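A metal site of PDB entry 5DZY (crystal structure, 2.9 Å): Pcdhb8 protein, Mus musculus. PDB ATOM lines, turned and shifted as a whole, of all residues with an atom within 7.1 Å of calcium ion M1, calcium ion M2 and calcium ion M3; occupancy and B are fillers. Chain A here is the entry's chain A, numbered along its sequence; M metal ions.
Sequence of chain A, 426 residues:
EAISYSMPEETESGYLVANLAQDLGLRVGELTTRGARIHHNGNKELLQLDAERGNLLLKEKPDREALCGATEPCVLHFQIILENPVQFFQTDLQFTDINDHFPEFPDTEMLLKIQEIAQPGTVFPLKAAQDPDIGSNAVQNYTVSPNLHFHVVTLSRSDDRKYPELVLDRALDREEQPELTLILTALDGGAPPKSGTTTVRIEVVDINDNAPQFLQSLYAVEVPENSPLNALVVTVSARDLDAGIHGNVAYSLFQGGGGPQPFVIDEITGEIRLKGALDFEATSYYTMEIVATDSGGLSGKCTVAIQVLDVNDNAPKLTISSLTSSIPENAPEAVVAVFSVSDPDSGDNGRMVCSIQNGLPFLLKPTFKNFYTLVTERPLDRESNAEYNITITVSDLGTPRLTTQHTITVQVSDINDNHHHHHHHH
Seven residues have an atom within 4 Å of calcium ion M2: Glu 9, Glu 65, Asp 97, Ile 98, Asp 100, His 101 and Asp 133.
Merely in contact with calcium ion M1: Glu 10 (3.6 Å).
Calcium ion M1 is bound by OD2 of Asp 100, 2.2 Å away.
Calcium ion M1 is bound by OD1 of Asp 63, at 2.5 Å.
OE1 of Glu 65 binds calcium ion M1, 2.7 Å away.
Calcium ion M1 has three donor atoms within binding distance.
Slightly farther from calcium ion M1 lies OE2 of Glu 9 (2.9 Å).
Slightly farther from calcium ion M1 lies NE2 of His 101 (3.0 Å).
Slightly farther from calcium ion M1 lies the side-chain carboxylate (OD1) of Asp 100 (3.1 Å).
The side-chain carboxylate (OD2) of Asp 131 is bound to calcium ion M3, at 2.2 Å.
OD2 of Asp 188 is bound to calcium ion M3.
The side-chain carboxylate (OD2) of Asp 133 binds calcium ion M3.
O of His 101 binds calcium ion M3 (2.5 Å).
OD1 of Asn 99 is bound to calcium ion M3, 2.5 Å away.
O of Asn 137 is bound to calcium ion M3 (2.7 Å).
Calcium ion M3 has six donor atoms within binding distance.
Slightly farther from calcium ion M3 lies the side-chain carboxylate (OD1) of Asp 131 (2.9 Å).
Calcium ion M2 is bound by OE2 of Glu 65, OD1 of Asp 100, OD1 of Asp 97, O of Ile 98, OD1 of Asp 133 and OE1 of Glu 9.
Calcium ion M2 has six donor atoms within binding distance.
Of the 28 residues printed, 6 come within 4 Å of calcium ion M3.
N of Asp 188 sits at hydrogen-bond distance from O of Lys 194 (2.8 Å).
OD1 of Asp 188 is in hydrogen-bond range of N of Gly 190 (3.0 Å).
The side-chain carboxylate (OE2) of Glu 65 lies close to the guanidinium group (NH1) of Arg 64.
OE2 of Glu 10 sits close to OD1 of Asp 63 (2.6 Å).
OD2 of Asp 97 sits at hydrogen-bond distance from ND2 of Asn 137.
The guanidinium group (NH1) of Arg 64 lies close to the side-chain carboxylate (OD1) of Asp 97, 3.1 Å away.
N of Glu 9 sits at hydrogen-bond distance from O of Thr 96 (2.8 Å).
N of Glu 10 sits at hydrogen-bond distance from O of Pro 62 (3.2 Å).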
ATOM      1  N   GLU A   9     -14.816 -23.951 -35.566  1.00  0.00           N
ATOM      2  CA  GLU A   9     -13.963 -25.118 -35.744  1.00  0.00           C
ATOM      3  C   GLU A   9     -14.723 -26.408 -35.439  1.00  0.00           C
ATOM      4  O   GLU A   9     -15.725 -26.400 -34.735  1.00  0.00           O
ATOM      5  CB  GLU A   9     -12.732 -25.005 -34.835  1.00  0.00           C
ATOM      6  CG  GLU A   9     -11.667 -26.072 -35.055  1.00  0.00           C
ATOM      7  CD  GLU A   9     -10.648 -26.117 -33.928  1.00  0.00           C
ATOM      8  OE1 GLU A   9     -10.689 -25.216 -33.052  1.00  0.00           O
ATOM      9  OE2 GLU A   9      -9.813 -27.037 -33.918  1.00  0.00           O
ATOM     10  N   GLU A  10     -14.237 -27.523 -35.995  1.00  0.00           N
ATOM     11  CA  GLU A  10     -14.768 -28.854 -35.716  1.00  0.00           C
ATOM     12  C   GLU A  10     -16.243 -28.997 -36.053  1.00  0.00           C
ATOM     13  O   GLU A  10     -16.982 -29.704 -35.370  1.00  0.00           O
ATOM     14  CB  GLU A  10     -14.539 -29.214 -34.240  1.00  0.00           C
ATOM     15  CG  GLU A  10     -13.076 -29.386 -33.848  1.00  0.00           C
ATOM     16  CD  GLU A  10     -12.497 -30.712 -34.296  1.00  0.00           C
ATOM     17  OE1 GLU A  10     -13.247 -31.539 -34.854  1.00  0.00           O
ATOM     18  OE2 GLU A  10     -11.285 -30.930 -34.082  1.00  0.00           O
ATOM     19  N   PRO A  62     -12.815 -30.051 -40.250  1.00  0.00           N
ATOM     20  CA  PRO A  62     -11.584 -29.273 -40.051  1.00  0.00           C
ATOM     21  C   PRO A  62     -11.164 -29.126 -38.589  1.00  0.00           C
ATOM     22  O   PRO A  62     -12.017 -29.018 -37.705  1.00  0.00           O
ATOM     23  CB  PRO A  62     -11.956 -27.907 -40.643  1.00  0.00           C
ATOM     24  CG  PRO A  62     -13.410 -27.789 -40.362  1.00  0.00           C
ATOM     25  CD  PRO A  62     -13.982 -29.179 -40.470  1.00  0.00           C
ATOM     26  N   ASP A  63      -9.855 -29.133 -38.353  1.00  0.00           N
ATOM     27  CA  ASP A  63      -9.306 -28.876 -37.025  1.00  0.00           C
ATOM     28  C   ASP A  63      -8.260 -27.777 -37.112  1.00  0.00           C
ATOM     29  O   ASP A  63      -7.226 -27.941 -37.760  1.00  0.00           O
ATOM     30  CB  ASP A  63      -8.693 -30.150 -36.445  1.00  0.00           C
ATOM     31  CG  ASP A  63      -8.090 -29.928 -35.063  1.00  0.00           C
ATOM     32  OD1 ASP A  63      -8.831 -30.019 -34.063  1.00  0.00           O
ATOM     33  OD2 ASP A  63      -6.869 -29.661 -34.993  1.00  0.00           O
ATOM     34  N   ARG A  64      -8.536 -26.655 -36.455  1.00  0.00           N
ATOM     35  CA  ARG A  64      -7.712 -25.451 -36.552  1.00  0.00           C
ATOM     36  C   ARG A  64      -6.250 -25.707 -36.185  1.00  0.00           C
ATOM     37  O   ARG A  64      -5.344 -25.292 -36.909  1.00  0.00           O
ATOM     38  CB  ARG A  64      -8.291 -24.350 -35.657  1.00  0.00           C
ATOM     39  CG  ARG A  64      -8.074 -22.919 -36.163  1.00  0.00           C
ATOM     40  CD  ARG A  64      -6.635 -22.463 -35.992  1.00  0.00           C
ATOM     41  NE  ARG A  64      -6.095 -22.855 -34.693  1.00  0.00           N
ATOM     42  CZ  ARG A  64      -6.252 -22.161 -33.574  1.00  0.00           C
ATOM     43  NH1 ARG A  64      -5.713 -22.595 -32.438  1.00  0.00           N
ATOM     44  NH2 ARG A  64      -6.944 -21.033 -33.582  1.00  0.00           N
ATOM     45  N   GLU A  65      -6.039 -26.386 -35.071  1.00  0.00           N
ATOM     46  CA  GLU A  65      -4.687 -26.621 -34.563  1.00  0.00           C
ATOM     47  C   GLU A  65      -3.842 -27.454 -35.517  1.00  0.00           C
ATOM     48  O   GLU A  65      -2.613 -27.368 -35.516  1.00  0.00           O
ATOM     49  CB  GLU A  65      -4.741 -27.299 -33.191  1.00  0.00           C
ATOM     50  CG  GLU A  65      -5.240 -26.403 -32.063  1.00  0.00           C
ATOM     51  CD  GLU A  65      -6.731 -26.146 -32.122  1.00  0.00           C
ATOM     52  OE1 GLU A  65      -7.478 -27.080 -32.490  1.00  0.00           O
ATOM     53  OE2 GLU A  65      -7.163 -25.015 -31.820  1.00  0.00           O
ATOM     54  N   ALA A  66      -4.499 -28.259 -36.342  1.00  0.00           N
ATOM     55  CA  ALA A  66      -3.809 -29.100 -37.314  1.00  0.00           C
ATOM     56  C   ALA A  66      -3.688 -28.400 -38.660  1.00  0.00           C
ATOM     57  O   ALA A  66      -2.905 -28.817 -39.523  1.00  0.00           O
ATOM     58  CB  ALA A  66      -4.522 -30.431 -37.468  1.00  0.00           C
ATOM     59  N   THR A  96     -13.149 -20.042 -37.032  1.00  0.00           N
ATOM     60  CA  THR A  96     -13.149 -19.533 -35.672  1.00  0.00           C
ATOM     61  C   THR A  96     -12.781 -20.646 -34.685  1.00  0.00           C
ATOM     62  O   THR A  96     -13.414 -21.696 -34.670  1.00  0.00           O
ATOM     63  CB  THR A  96     -14.512 -18.939 -35.276  1.00  0.00           C
ATOM     64  OG1 THR A  96     -14.784 -17.797 -36.101  1.00  0.00           O
ATOM     65  CG2 THR A  96     -14.517 -18.508 -33.819  1.00  0.00           C
ATOM     66  N   ASP A  97     -11.753 -20.389 -33.874  1.00  0.00           N
ATOM     67  CA  ASP A  97     -11.277 -21.389 -32.923  1.00  0.00           C
ATOM     68  C   ASP A  97     -12.300 -21.641 -31.815  1.00  0.00           C
ATOM     69  O   ASP A  97     -12.951 -20.722 -31.334  1.00  0.00           O
ATOM     70  CB  ASP A  97      -9.947 -20.934 -32.308  1.00  0.00           C
ATOM     71  CG  ASP A  97      -9.440 -21.902 -31.260  1.00  0.00           C
ATOM     72  OD1 ASP A  97      -8.663 -22.818 -31.620  1.00  0.00           O
ATOM     73  OD2 ASP A  97      -9.808 -21.749 -30.075  1.00  0.00           O
ATOM     74  N   ILE A  98     -12.414 -22.908 -31.420  1.00  0.00           N
ATOM     75  CA  ILE A  98     -13.286 -23.284 -30.314  1.00  0.00           C
ATOM     76  C   ILE A  98     -12.468 -23.865 -29.165  1.00  0.00           C
ATOM     77  O   ILE A  98     -11.322 -24.275 -29.355  1.00  0.00           O
ATOM     78  CB  ILE A  98     -14.351 -24.319 -30.750  1.00  0.00           C
ATOM     79  CG1 ILE A  98     -13.678 -25.623 -31.167  1.00  0.00           C
ATOM     80  CG2 ILE A  98     -15.203 -23.755 -31.876  1.00  0.00           C
ATOM     81  CD1 ILE A  98     -14.655 -26.729 -31.509  1.00  0.00           C
ATOM     82  N   ASN A  99     -13.054 -23.886 -27.974  1.00  0.00           N
ATOM     83  CA  ASN A  99     -12.377 -24.430 -26.809  1.00  0.00           C
ATOM     84  C   ASN A  99     -12.554 -25.948 -26.728  1.00  0.00           C
ATOM     85  O   ASN A  99     -13.311 -26.443 -25.889  1.00  0.00           O
ATOM     86  CB  ASN A  99     -12.887 -23.766 -25.527  1.00  0.00           C
ATOM     87  CG  ASN A  99     -12.070 -24.135 -24.304  1.00  0.00           C
ATOM     88  OD1 ASN A  99     -10.931 -24.577 -24.426  1.00  0.00           O
ATOM     89  ND2 ASN A  99     -12.653 -23.956 -23.125  1.00  0.00           N
ATOM     90  N   ASP A 100     -11.870 -26.666 -27.602  1.00  0.00           N
ATOM     91  CA  ASP A 100     -11.989 -28.123 -27.663  1.00  0.00           C
ATOM     92  C   ASP A 100     -10.715 -28.815 -27.196  1.00  0.00           C
ATOM     93  O   ASP A 100     -10.481 -29.983 -27.521  1.00  0.00           O
ATOM     94  CB  ASP A 100     -12.353 -28.558 -29.081  1.00  0.00           C
ATOM     95  CG  ASP A 100     -11.352 -28.065 -30.117  1.00  0.00           C
ATOM     96  OD1 ASP A 100     -10.617 -27.100 -29.829  1.00  0.00           O
ATOM     97  OD2 ASP A 100     -11.313 -28.642 -31.219  1.00  0.00           O
ATOM     98  N   HIS A 101      -9.891 -28.096 -26.448  1.00  0.00           N
ATOM     99  CA  HIS A 101      -8.656 -28.655 -25.898  1.00  0.00           C
ATOM    100  C   HIS A 101      -8.585 -28.452 -24.394  1.00  0.00           C
ATOM    101  O   HIS A 101      -8.739 -27.325 -23.901  1.00  0.00           O
ATOM    102  CB  HIS A 101      -7.434 -28.041 -26.575  1.00  0.00           C
ATOM    103  CG  HIS A 101      -7.084 -28.665 -27.889  1.00  0.00           C
ATOM    104  ND1 HIS A 101      -6.168 -29.686 -28.016  1.00  0.00           N
ATOM    105  CD2 HIS A 101      -7.540 -28.411 -29.143  1.00  0.00           C
ATOM    106  CE1 HIS A 101      -6.072 -30.035 -29.290  1.00  0.00           C
ATOM    107  NE2 HIS A 101      -6.891 -29.275 -29.990  1.00  0.00           N
ATOM    108  N   PHE A 102      -8.361 -29.533 -23.653  1.00  0.00           N
ATOM    109  CA  PHE A 102      -8.198 -29.451 -22.208  1.00  0.00           C
ATOM    110  C   PHE A 102      -6.756 -29.103 -21.846  1.00  0.00           C
ATOM    111  O   PHE A 102      -5.827 -29.630 -22.445  1.00  0.00           O
ATOM    112  CB  PHE A 102      -8.608 -30.766 -21.541  1.00  0.00           C
ATOM    113  CG  PHE A 102     -10.088 -31.003 -21.517  1.00  0.00           C
ATOM    114  CD1 PHE A 102     -10.978 -29.972 -21.780  1.00  0.00           C
ATOM    115  CD2 PHE A 102     -10.595 -32.260 -21.213  1.00  0.00           C
ATOM    116  CE1 PHE A 102     -12.344 -30.192 -21.748  1.00  0.00           C
ATOM    117  CE2 PHE A 102     -11.961 -32.480 -21.182  1.00  0.00           C
ATOM    118  CZ  PHE A 102     -12.828 -31.441 -21.449  1.00  0.00           C
ATOM    119  N   PRO A 103      -6.582 -28.213 -20.858  1.00  0.00           N
ATOM    120  CA  PRO A 103      -5.251 -27.863 -20.353  1.00  0.00           C
ATOM    121  C   PRO A 103      -4.508 -29.098 -19.838  1.00  0.00           C
ATOM    122  O   PRO A 103      -5.036 -29.821 -18.992  1.00  0.00           O
ATOM    123  CB  PRO A 103      -5.551 -26.889 -19.207  1.00  0.00           C
ATOM    124  CG  PRO A 103      -6.879 -26.311 -19.553  1.00  0.00           C
ATOM    125  CD  PRO A 103      -7.644 -27.424 -20.213  1.00  0.00           C
ATOM    126  N   GLN A 130      -0.110 -26.236 -20.758  1.00  0.00           N
ATOM    127  CA  GLN A 130      -0.149 -25.842 -22.168  1.00  0.00           C
ATOM    128  C   GLN A 130      -1.531 -26.053 -22.776  1.00  0.00           C
ATOM    129  O   GLN A 130      -2.252 -26.985 -22.416  1.00  0.00           O
ATOM    130  CB  GLN A 130       0.906 -26.619 -22.955  1.00  0.00           C
ATOM    131  CG  GLN A 130       2.335 -26.313 -22.532  1.00  0.00           C
ATOM    132  CD  GLN A 130       3.359 -27.108 -23.308  1.00  0.00           C
ATOM    133  OE1 GLN A 130       3.033 -28.101 -23.957  1.00  0.00           O
ATOM    134  NE2 GLN A 130       4.615 -26.680 -23.231  1.00  0.00           N
ATOM    135  N   ASP A 131      -1.889 -25.175 -23.708  1.00  0.00           N
ATOM    136  CA  ASP A 131      -3.186 -25.244 -24.375  1.00  0.00           C
ATOM    137  C   ASP A 131      -3.062 -24.757 -25.807  1.00  0.00           C
ATOM    138  O   ASP A 131      -2.791 -23.577 -26.055  1.00  0.00           O
ATOM    139  CB  ASP A 131      -4.215 -24.400 -23.614  1.00  0.00           C
ATOM    140  CG  ASP A 131      -5.646 -24.839 -23.887  1.00  0.00           C
ATOM    141  OD1 ASP A 131      -5.916 -25.328 -25.001  1.00  0.00           O
ATOM    142  OD2 ASP A 131      -6.495 -24.688 -22.987  1.00  0.00           O
ATOM    143  N   PRO A 132      -3.262 -25.674 -26.775  1.00  0.00           N
ATOM    144  CA  PRO A 132      -3.116 -25.400 -28.211  1.00  0.00           C
ATOM    145  C   PRO A 132      -4.099 -24.362 -28.750  1.00  0.00           C
ATOM    146  O   PRO A 132      -3.975 -23.951 -29.909  1.00  0.00           O
ATOM    147  CB  PRO A 132      -3.376 -26.768 -28.861  1.00  0.00           C
ATOM    148  CG  PRO A 132      -3.110 -27.754 -27.774  1.00  0.00           C
ATOM    149  CD  PRO A 132      -3.556 -27.095 -26.521  1.00  0.00           C
ATOM    150  N   ASP A 133      -5.067 -23.946 -27.932  1.00  0.00           N
ATOM    151  CA  ASP A 133      -6.068 -22.984 -28.355  1.00  0.00           C
ATOM    152  C   ASP A 133      -5.499 -21.574 -28.477  1.00  0.00           C
ATOM    153  O   ASP A 133      -4.300 -21.358 -28.266  1.00  0.00           O
ATOM    154  CB  ASP A 133      -7.244 -22.976 -27.381  1.00  0.00           C
ATOM    155  CG  ASP A 133      -7.885 -24.350 -27.229  1.00  0.00           C
ATOM    156  OD1 ASP A 133      -7.818 -25.143 -28.194  1.00  0.00           O
ATOM    157  OD2 ASP A 133      -8.440 -24.628 -26.150  1.00  0.00           O
ATOM    158  N   ILE A 134      -6.351 -20.615 -28.817  1.00  0.00           N
ATOM    159  CA  ILE A 134      -5.923 -19.231 -29.023  1.00  0.00           C
ATOM    160  C   ILE A 134      -6.849 -18.238 -28.333  1.00  0.00           C
ATOM    161  O   ILE A 134      -8.070 -18.312 -28.473  1.00  0.00           O
ATOM    162  CB  ILE A 134      -5.840 -18.884 -30.532  1.00  0.00           C
ATOM    163  CG1 ILE A 134      -4.675 -19.638 -31.189  1.00  0.00           C
ATOM    164  CG2 ILE A 134      -5.687 -17.392 -30.738  1.00  0.00           C
ATOM    165  CD1 ILE A 134      -4.394 -19.195 -32.611  1.00  0.00           C
ATOM    166  N   SER A 136      -8.988 -16.388 -25.574  1.00  0.00           N
ATOM    167  CA  SER A 136      -9.757 -16.715 -24.373  1.00  0.00           C
ATOM    168  C   SER A 136      -9.916 -18.222 -24.210  1.00  0.00           C
ATOM    169  O   SER A 136     -10.207 -18.708 -23.113  1.00  0.00           O
ATOM    170  CB  SER A 136     -11.125 -16.037 -24.428  1.00  0.00           C
ATOM    171  OG  SER A 136     -11.873 -16.328 -23.256  1.00  0.00           O
ATOM    172  N   ASN A 137      -9.707 -18.954 -25.299  1.00  0.00           N
ATOM    173  CA  ASN A 137      -9.815 -20.410 -25.271  1.00  0.00           C
ATOM    174  C   ASN A 137      -8.544 -21.062 -24.723  1.00  0.00           C
ATOM    175  O   ASN A 137      -8.502 -22.277 -24.520  1.00  0.00           O
ATOM    176  CB  ASN A 137     -10.118 -20.946 -26.670  1.00  0.00           C
ATOM    177  CG  ASN A 137     -11.461 -20.480 -27.186  1.00  0.00           C
ATOM    178  OD1 ASN A 137     -12.413 -20.293 -26.414  1.00  0.00           O
ATOM    179  ND2 ASN A 137     -11.558 -20.304 -28.499  1.00  0.00           N
ATOM    180  N   ALA A 138      -7.516 -20.254 -24.490  1.00  0.00           N
ATOM    181  CA  ALA A 138      -6.257 -20.744 -23.952  1.00  0.00           C
ATOM    182  C   ALA A 138      -6.234 -20.649 -22.429  1.00  0.00           C
ATOM    183  O   ALA A 138      -7.256 -20.377 -21.800  1.00  0.00           O
ATOM    184  CB  ALA A 138      -5.088 -19.978 -24.551  1.00  0.00           C
ATOM    185  N   VAL A 139      -5.072 -20.889 -21.843  1.00  0.00           N
ATOM    186  CA  VAL A 139      -4.918 -20.816 -20.391  1.00  0.00           C
ATOM    187  C   VAL A 139      -5.162 -19.402 -19.883  1.00  0.00           C
ATOM    188  O   VAL A 139      -4.654 -18.428 -20.432  1.00  0.00           O
ATOM    189  CB  VAL A 139      -3.515 -21.283 -19.950  1.00  0.00           C
ATOM    190  CG1 VAL A 139      -3.439 -22.797 -19.940  1.00  0.00           C
ATOM    191  CG2 VAL A 139      -2.441 -20.694 -20.851  1.00  0.00           C
ATOM    192  N   ASP A 188      -9.404 -22.596 -17.828  1.00  0.00           N
ATOM    193  CA  ASP A 188      -9.518 -21.943 -19.123  1.00  0.00           C
ATOM    194  C   ASP A 188     -10.408 -20.713 -19.012  1.00  0.00           C
ATOM    195  O   ASP A 188     -11.161 -20.568 -18.054  1.00  0.00           O
ATOM    196  CB  ASP A 188     -10.072 -22.930 -20.164  1.00  0.00           C
ATOM    197  CG  ASP A 188      -9.832 -22.486 -21.595  1.00  0.00           C
ATOM    198  OD1 ASP A 188      -9.923 -21.269 -21.874  1.00  0.00           O
ATOM    199  OD2 ASP A 188      -9.552 -23.350 -22.439  1.00  0.00           O
ATOM    200  N   GLY A 189     -10.327 -19.825 -20.004  1.00  0.00           N
ATOM    201  CA  GLY A 189     -11.127 -18.613 -20.010  1.00  0.00           C
ATOM    202  C   GLY A 189     -12.358 -18.731 -20.883  1.00  0.00           C
ATOM    203  O   GLY A 189     -13.107 -17.765 -21.063  1.00  0.00           O
ATOM    204  N   GLY A 190     -12.571 -19.918 -21.452  1.00  0.00           N
ATOM    205  CA  GLY A 190     -13.703 -20.159 -22.317  1.00  0.00           C
ATOM    206  C   GLY A 190     -14.975 -20.436 -21.536  1.00  0.00           C
ATOM    207  O   GLY A 190     -14.976 -20.468 -20.307  1.00  0.00           O
ATOM    208  N   LYS A 194     -12.426 -24.963 -19.163  1.00  0.00           N
ATOM    209  CA  LYS A 194     -11.829 -26.285 -19.120  1.00  0.00           C
ATOM    210  C   LYS A 194     -10.692 -26.318 -18.108  1.00  0.00           C
ATOM    211  O   LYS A 194      -9.978 -25.337 -17.929  1.00  0.00           O
ATOM    212  CB  LYS A 194     -11.310 -26.682 -20.509  1.00  0.00           C
HETATM  213 CA    CA M   1      -9.195 -29.005 -31.835  1.00  0.00          CA
HETATM  214 CA    CA M   2      -9.241 -25.113 -30.615  1.00  0.00          CA
HETATM  215 CA    CA M   3      -8.538 -24.863 -23.849  1.00  0.00          CA
